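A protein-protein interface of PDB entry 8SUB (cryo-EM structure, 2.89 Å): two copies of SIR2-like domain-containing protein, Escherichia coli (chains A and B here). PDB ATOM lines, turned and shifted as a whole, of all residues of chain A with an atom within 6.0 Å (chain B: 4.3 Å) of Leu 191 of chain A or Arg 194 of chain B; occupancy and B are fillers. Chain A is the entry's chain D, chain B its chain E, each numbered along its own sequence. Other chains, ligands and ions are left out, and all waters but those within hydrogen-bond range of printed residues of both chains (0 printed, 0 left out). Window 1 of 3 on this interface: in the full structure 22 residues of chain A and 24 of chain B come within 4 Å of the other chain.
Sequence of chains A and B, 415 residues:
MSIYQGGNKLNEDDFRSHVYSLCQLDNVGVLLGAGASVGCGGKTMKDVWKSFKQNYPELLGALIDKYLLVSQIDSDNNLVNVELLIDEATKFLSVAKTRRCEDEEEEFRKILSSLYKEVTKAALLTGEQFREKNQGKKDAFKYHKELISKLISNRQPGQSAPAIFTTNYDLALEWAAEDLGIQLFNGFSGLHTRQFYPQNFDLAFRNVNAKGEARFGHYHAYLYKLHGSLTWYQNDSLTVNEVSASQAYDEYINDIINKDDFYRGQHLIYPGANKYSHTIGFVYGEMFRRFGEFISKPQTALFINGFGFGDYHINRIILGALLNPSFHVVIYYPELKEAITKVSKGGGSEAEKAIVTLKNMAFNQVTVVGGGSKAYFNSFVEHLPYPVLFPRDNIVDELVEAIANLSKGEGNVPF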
ATOM      1  N   LYS A 133      30.458  16.995  -1.883  1.00  0.00           N
ATOM      2  CA  LYS A 133      29.204  16.375  -2.279  1.00  0.00           C
ATOM      3  C   LYS A 133      28.909  16.651  -3.748  1.00  0.00           C
ATOM      4  O   LYS A 133      29.489  17.544  -4.366  1.00  0.00           O
ATOM      5  CB  LYS A 133      28.052  16.886  -1.415  1.00  0.00           C
ATOM      6  CG  LYS A 133      28.032  16.340  -0.008  1.00  0.00           C
ATOM      7  CD  LYS A 133      26.798  16.820   0.732  1.00  0.00           C
ATOM      8  CE  LYS A 133      26.766  16.291   2.148  1.00  0.00           C
ATOM      9  NZ  LYS A 133      26.493  14.830   2.178  1.00  0.00           N
ATOM     10  N   SER A 189      23.945  -2.790   5.007  1.00  0.00           N
ATOM     11  CA  SER A 189      22.669  -2.275   5.491  1.00  0.00           C
ATOM     12  C   SER A 189      22.894  -1.439   6.745  1.00  0.00           C
ATOM     13  O   SER A 189      23.749  -1.761   7.570  1.00  0.00           O
ATOM     14  CB  SER A 189      21.695  -3.418   5.777  1.00  0.00           C
ATOM     15  OG  SER A 189      20.435  -2.932   6.191  1.00  0.00           O
ATOM     16  N   GLY A 190      22.110  -0.375   6.885  1.00  0.00           N
ATOM     17  CA  GLY A 190      22.183   0.511   8.029  1.00  0.00           C
ATOM     18  C   GLY A 190      22.864   1.828   7.697  1.00  0.00           C
ATOM     19  O   GLY A 190      23.524   1.987   6.672  1.00  0.00           O
ATOM     20  N   LEU A 191      22.681   2.808   8.584  1.00  0.00           N
ATOM     21  CA  LEU A 191      23.333   4.106   8.425  1.00  0.00           C
ATOM     22  C   LEU A 191      24.267   4.434   9.581  1.00  0.00           C
ATOM     23  O   LEU A 191      25.432   4.763   9.345  1.00  0.00           O
ATOM     24  CB  LEU A 191      22.290   5.217   8.260  1.00  0.00           C
ATOM     25  CG  LEU A 191      22.836   6.647   8.297  1.00  0.00           C
ATOM     26  CD1 LEU A 191      23.794   6.873   7.154  1.00  0.00           C
ATOM     27  CD2 LEU A 191      21.721   7.654   8.235  1.00  0.00           C
ATOM     28  N   HIS A 192      23.792   4.370  10.826  1.00  0.00           N
ATOM     29  CA  HIS A 192      24.640   4.744  11.955  1.00  0.00           C
ATOM     30  C   HIS A 192      25.687   3.678  12.246  1.00  0.00           C
ATOM     31  O   HIS A 192      26.801   4.005  12.667  1.00  0.00           O
ATOM     32  CB  HIS A 192      23.778   5.023  13.185  1.00  0.00           C
ATOM     33  CG  HIS A 192      22.771   6.112  12.977  1.00  0.00           C
ATOM     34  ND1 HIS A 192      23.102   7.448  12.996  1.00  0.00           N
ATOM     35  CD2 HIS A 192      21.443   6.057  12.725  1.00  0.00           C
ATOM     36  CE1 HIS A 192      22.020   8.170  12.770  1.00  0.00           C
ATOM     37  NE2 HIS A 192      21.001   7.351  12.598  1.00  0.00           N
ATOM     38  N   THR A 193      25.352   2.407  12.029  1.00  0.00           N
ATOM     39  CA  THR A 193      26.326   1.315  12.034  1.00  0.00           C
ATOM     40  C   THR A 193      26.019   0.446  10.818  1.00  0.00           C
ATOM     41  O   THR A 193      25.067  -0.337  10.834  1.00  0.00           O
ATOM     42  CB  THR A 193      26.276   0.512  13.326  1.00  0.00           C
ATOM     43  OG1 THR A 193      26.220   1.407  14.442  1.00  0.00           O
ATOM     44  CG2 THR A 193      27.514  -0.344  13.461  1.00  0.00           C
ATOM     45  N   ARG A 194      26.827   0.595   9.771  1.00  0.00           N
ATOM     46  CA  ARG A 194      26.636  -0.094   8.500  1.00  0.00           C
ATOM     47  C   ARG A 194      27.438  -1.393   8.496  1.00  0.00           C
ATOM     48  O   ARG A 194      28.644  -1.379   8.754  1.00  0.00           O
ATOM     49  CB  ARG A 194      27.061   0.836   7.360  1.00  0.00           C
ATOM     50  CG  ARG A 194      27.038   0.247   5.970  1.00  0.00           C
ATOM     51  CD  ARG A 194      25.654   0.050   5.441  1.00  0.00           C
ATOM     52  NE  ARG A 194      25.026   1.249   4.903  1.00  0.00           N
ATOM     53  CZ  ARG A 194      24.936   1.530   3.611  1.00  0.00           C
ATOM     54  NH1 ARG A 194      25.511   0.774   2.695  1.00  0.00           N
ATOM     55  NH2 ARG A 194      24.234   2.589   3.227  1.00  0.00           N
ATOM     56  N   GLU A 242      31.125  -0.158   6.385  1.00  0.00           N
ATOM     57  CA  GLU A 242      31.219   0.819   5.312  1.00  0.00           C
ATOM     58  C   GLU A 242      30.934   2.215   5.848  1.00  0.00           C
ATOM     59  O   GLU A 242      30.196   2.391   6.818  1.00  0.00           O
ATOM     60  CB  GLU A 242      30.246   0.500   4.180  1.00  0.00           C
ATOM     61  CG  GLU A 242      30.497   1.308   2.923  1.00  0.00           C
ATOM     62  CD  GLU A 242      29.465   1.079   1.851  1.00  0.00           C
ATOM     63  OE1 GLU A 242      28.413   0.492   2.153  1.00  0.00           O
ATOM     64  OE2 GLU A 242      29.705   1.489   0.701  1.00  0.00           O
ATOM     65  N   GLU B 178      18.649  -0.959  14.573  1.00  0.00           N
ATOM     66  CA  GLU B 178      19.869  -1.403  13.906  1.00  0.00           C
ATOM     67  C   GLU B 178      20.571  -2.533  14.643  1.00  0.00           C
ATOM     68  O   GLU B 178      21.506  -3.117  14.093  1.00  0.00           O
ATOM     69  CB  GLU B 178      20.835  -0.236  13.729  1.00  0.00           C
ATOM     70  CG  GLU B 178      20.595   0.570  12.475  1.00  0.00           C
ATOM     71  CD  GLU B 178      21.480   1.788  12.392  1.00  0.00           C
ATOM     72  OE1 GLU B 178      22.430   1.881  13.189  1.00  0.00           O
ATOM     73  OE2 GLU B 178      21.226   2.659  11.536  1.00  0.00           O
ATOM     74  N   ASN B 186      12.316   5.621   6.127  1.00  0.00           N
ATOM     75  CA  ASN B 186      12.012   6.958   6.625  1.00  0.00           C
ATOM     76  C   ASN B 186      12.070   8.038   5.548  1.00  0.00           C
ATOM     77  O   ASN B 186      12.122   9.223   5.893  1.00  0.00           O
ATOM     78  CB  ASN B 186      12.945   7.332   7.784  1.00  0.00           C
ATOM     79  CG  ASN B 186      14.396   7.422   7.367  1.00  0.00           C
ATOM     80  OD1 ASN B 186      14.858   6.667   6.519  1.00  0.00           O
ATOM     81  ND2 ASN B 186      15.128   8.347   7.970  1.00  0.00           N
ATOM     82  N   PHE B 188      14.427   8.623   3.056  1.00  0.00           N
ATOM     83  CA  PHE B 188      15.728   9.051   2.563  1.00  0.00           C
ATOM     84  C   PHE B 188      16.442   7.883   1.896  1.00  0.00           C
ATOM     85  O   PHE B 188      16.240   6.725   2.268  1.00  0.00           O
ATOM     86  CB  PHE B 188      16.593   9.611   3.694  1.00  0.00           C
ATOM     87  CG  PHE B 188      16.226  11.008   4.115  1.00  0.00           C
ATOM     88  CD1 PHE B 188      15.113  11.239   4.894  1.00  0.00           C
ATOM     89  CD2 PHE B 188      17.001  12.084   3.744  1.00  0.00           C
ATOM     90  CE1 PHE B 188      14.776  12.511   5.281  1.00  0.00           C
ATOM     91  CE2 PHE B 188      16.663  13.358   4.130  1.00  0.00           C
ATOM     92  CZ  PHE B 188      15.552  13.569   4.900  1.00  0.00           C
ATOM     93  N   SER B 189      17.280   8.186   0.902  1.00  0.00           N
ATOM     94  CA  SER B 189      17.996   7.150   0.168  1.00  0.00           C
ATOM     95  C   SER B 189      19.338   7.670  -0.328  1.00  0.00           C
ATOM     96  O   SER B 189      19.419   8.775  -0.865  1.00  0.00           O
ATOM     97  CB  SER B 189      17.169   6.648  -1.014  1.00  0.00           C
ATOM     98  OG  SER B 189      15.986   6.018  -0.565  1.00  0.00           O
ATOM     99  N   GLY B 190      20.375   6.859  -0.177  1.00  0.00           N
ATOM    100  CA  GLY B 190      21.723   7.216  -0.571  1.00  0.00           C
ATOM    101  C   GLY B 190      22.737   6.907   0.516  1.00  0.00           C
ATOM    102  O   GLY B 190      22.409   6.437   1.602  1.00  0.00           O
ATOM    103  N   LEU B 191      24.002   7.109   0.168  1.00  0.00           N
ATOM    104  CA  LEU B 191      25.023   7.122   1.215  1.00  0.00           C
ATOM    105  C   LEU B 191      25.974   8.304   1.122  1.00  0.00           C
ATOM    106  O   LEU B 191      26.242   8.949   2.134  1.00  0.00           O
ATOM    107  CB  LEU B 191      25.833   5.821   1.202  1.00  0.00           C
ATOM    108  CG  LEU B 191      27.015   5.721   2.173  1.00  0.00           C
ATOM    109  CD1 LEU B 191      26.596   5.981   3.600  1.00  0.00           C
ATOM    110  CD2 LEU B 191      27.645   4.363   2.069  1.00  0.00           C
ATOM    111  N   THR B 193      25.420  11.036  -0.812  1.00  0.00           N
ATOM    112  CA  THR B 193      24.490  12.152  -0.630  1.00  0.00           C
ATOM    113  C   THR B 193      23.125  11.564  -0.295  1.00  0.00           C
ATOM    114  O   THR B 193      22.536  10.877  -1.132  1.00  0.00           O
ATOM    115  CB  THR B 193      24.392  13.032  -1.875  1.00  0.00           C
ATOM    116  OG1 THR B 193      24.120  12.215  -3.016  1.00  0.00           O
ATOM    117  CG2 THR B 193      25.659  13.822  -2.115  1.00  0.00           C
ATOM    118  N   ARG B 194      22.636  11.801   0.923  1.00  0.00           N
ATOM    119  CA  ARG B 194      21.263  11.448   1.273  1.00  0.00           C
ATOM    120  C   ARG B 194      20.295  12.512   0.776  1.00  0.00           C
ATOM    121  O   ARG B 194      20.574  13.709   0.863  1.00  0.00           O
ATOM    122  CB  ARG B 194      21.107  11.290   2.784  1.00  0.00           C
ATOM    123  CG  ARG B 194      21.892  10.169   3.392  1.00  0.00           C
ATOM    124  CD  ARG B 194      21.330   8.878   2.933  1.00  0.00           C
ATOM    125  NE  ARG B 194      20.083   8.514   3.590  1.00  0.00           N
ATOM    126  CZ  ARG B 194      19.975   7.569   4.511  1.00  0.00           C
ATOM    127  NH1 ARG B 194      21.019   6.861   4.894  1.00  0.00           N
ATOM    128  NH2 ARG B 194      18.785   7.305   5.036  1.00  0.00           N
ATOM    129  N   GLN B 195      19.152  12.076   0.251  1.00  0.00           N
ATOM    130  CA  GLN B 195      18.139  13.005  -0.222  1.00  0.00           C
ATOM    131  C   GLN B 195      16.744  12.499   0.115  1.00  0.00           C
ATOM    132  O   GLN B 195      16.514  11.294   0.228  1.00  0.00           O
ATOM    133  CB  GLN B 195      18.249  13.240  -1.724  1.00  0.00           C
ATOM    134  CG  GLN B 195      19.411  14.113  -2.119  1.00  0.00           C
ATOM    135  CD  GLN B 195      19.251  14.682  -3.503  1.00  0.00           C
ATOM    136  OE1 GLN B 195      18.146  14.730  -4.038  1.00  0.00           O
ATOM    137  NE2 GLN B 195      20.351  15.128  -4.089  1.00  0.00           N
ATOM    138  N   VAL B 240      17.358  18.871   1.039  1.00  0.00           N
ATOM    139  CA  VAL B 240      17.510  18.449   2.426  1.00  0.00           C
ATOM    140  C   VAL B 240      18.395  17.209   2.473  1.00  0.00           C
ATOM    141  O   VAL B 240      18.197  16.267   1.701  1.00  0.00           O
ATOM    142  CB  VAL B 240      16.138  18.182   3.065  1.00  0.00           C
ATOM    143  CG1 VAL B 240      16.290  17.508   4.415  1.00  0.00           C
ATOM    144  CG2 VAL B 240      15.360  19.478   3.194  1.00  0.00           C
ATOM    145  N   ASN B 241      19.379  17.214   3.371  1.00  0.00           N
ATOM    146  CA  ASN B 241      20.336  16.126   3.502  1.00  0.00           C
ATOM    147  C   ASN B 241      20.218  15.454   4.863  1.00  0.00           C
ATOM    148  O   ASN B 241      19.654  16.003   5.811  1.00  0.00           O
ATOM    149  CB  ASN B 241      21.776  16.617   3.315  1.00  0.00           C
ATOM    150  CG  ASN B 241      22.079  17.007   1.894  1.00  0.00           C
ATOM    151  OD1 ASN B 241      22.551  18.108   1.629  1.00  0.00           O
ATOM    152  ND2 ASN B 241      21.803  16.107   0.964  1.00  0.00           N
ATOM    153  N   GLU B 242      20.766  14.247   4.940  1.00  0.00           N
ATOM    154  CA  GLU B 242      20.877  13.487   6.174  1.00  0.00           C
ATOM    155  C   GLU B 242      22.286  12.932   6.286  1.00  0.00           C
ATOM    156  O   GLU B 242      22.864  12.489   5.292  1.00  0.00           O
ATOM    157  CB  GLU B 242      19.863  12.353   6.209  1.00  0.00           C
ATOM    158  CG  GLU B 242      19.765  11.651   7.535  1.00  0.00           C
ATOM    159  CD  GLU B 242      18.943  10.387   7.465  1.00  0.00           C
ATOM    160  OE1 GLU B 242      18.976   9.706   6.425  1.00  0.00           O
ATOM    161  OE2 GLU B 242      18.259  10.067   8.453  1.00  0.00           O
ATOM    162  N   VAL B 243      22.843  12.959   7.493  1.00  0.00           N
ATOM    163  CA  VAL B 243      24.180  12.456   7.757  1.00  0.00           C
ATOM    164  C   VAL B 243      24.103  11.456   8.902  1.00  0.00           C
ATOM    165  O   VAL B 243      23.028  11.121   9.387  1.00  0.00           O
ATOM    166  CB  VAL B 243      25.183  13.584   8.072  1.00  0.00           C
ATOM    167  CG1 VAL B 243      25.517  14.359   6.821  1.00  0.00           C
ATOM    168  CG2 VAL B 243      24.630  14.510   9.124  1.00  0.00           C
ATOM    169  N   SER B 244      25.260  10.963   9.311  1.00  0.00           N
ATOM    170  CA  SER B 244      25.366  10.062  10.446  1.00  0.00           C
ATOM    171  C   SER B 244      25.648  10.855  11.718  1.00  0.00           C
ATOM    172  O   SER B 244      26.001  12.033  11.673  1.00  0.00           O
ATOM    173  CB  SER B 244      26.460   9.028  10.193  1.00  0.00           C
ATOM    174  OG  SER B 244      26.727   8.281  11.354  1.00  0.00           O
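N of Leu 191 of chain A lies within hydrogen-bond range of OE2 of Glu 178 of chain B (3.3 Å). The backbone NH (N) of His 192 of chain A is in hydrogen-bond range of the side-chain carboxylate (OE2) of Glu 178 of chain B (3.2 Å). N of Thr 193 of chain A sits at hydrogen-bond distance from OE1 of Glu 178 of chain B (3.2 Å).
O of Arg 194 of chain B is in hydrogen-bond range of ND2 of Asn 241 of chain B (2.7 Å). The side-chain carboxylate (OE1) of Glu 242 of chain A lies within salt-bridge range of the guanidinium group (NH1) of Arg 194 of chain A (3.0 Å). NH2 of Arg 194 of chain B is in salt-bridge range of OE1 of Glu 242 of chain B (2.8 Å).
Among the printed residues, pairs that only touch across the chains: Leu 191 of chain A with Arg 194 of chain B (3.5 Å), Glu 242 of chain A with Leu 191 of chain B (3.8 Å), Leu 191 of chain A with Glu 242 of chain B (3.9 Å), Leu 191 of chain A with Val 243 of chain B (3.9 Å) and Lys 133 of chain A with Thr 193 of chain B (3.95 Å).
Leu 191 of chain A touches just these residues of chain B: Glu 178 (3.3 Å), Arg 194 (3.5 Å), Glu 242 (3.9 Å) and Val 243 (3.9 Å). Of the printed residues of chain B, His 192 of chain A touches Glu 178 (3.2 Å). Of the printed residues of chain B, Glu 242 of chain A touches Leu 191. Of the printed residues of chain A, Glu 178 of chain B touches Leu 191 (3.3 Å), His 192 (3.2 Å) and Thr 193 (3.2 Å). Printed residues of chain A within 4 Å of Leu 191 of chain B: Glu 242 (3.8 Å). Arg 194 of chain B touches just one residue of chain A: Leu 191. Gln 195 of chain B touches none of the printed residues of chain A. The nearest printed residue of chain B that does not touch Leu 191 of chain A is Ser 244 of chain B (4.3 Å).
Hydrophobic or aromatic side chains of chain B that line the printed part of chain A: Leu 191. Of the 8 printed residues of chain A, 5 touch a printed residue of chain B. Printed residues of chain A that touch a printed residue of chain B: Lys 133, Leu 191, His 192, Thr 193 and Glu 242. Among the printed residues, 8 pairs touch across the chains. Among the printed residues, no Asp or Glu carboxylate lies within 4 Å of a Lys or Arg side-chain nitrogen of the other chain.
Leu 191 of chain A touches Arg 194 of chain B, but with the chains exchanged Arg 194 of chain A does not touch Leu 191 of chain B (4.02 Å). Leu 191 of chain A touches Glu 242 of chain B, and with the chains exchanged Glu 242 of chain A touches Leu 191 of chain B. Of the 8 pairs that touch across the chains among the printed residues, 2 have their exchanged pair printed and touching as well.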
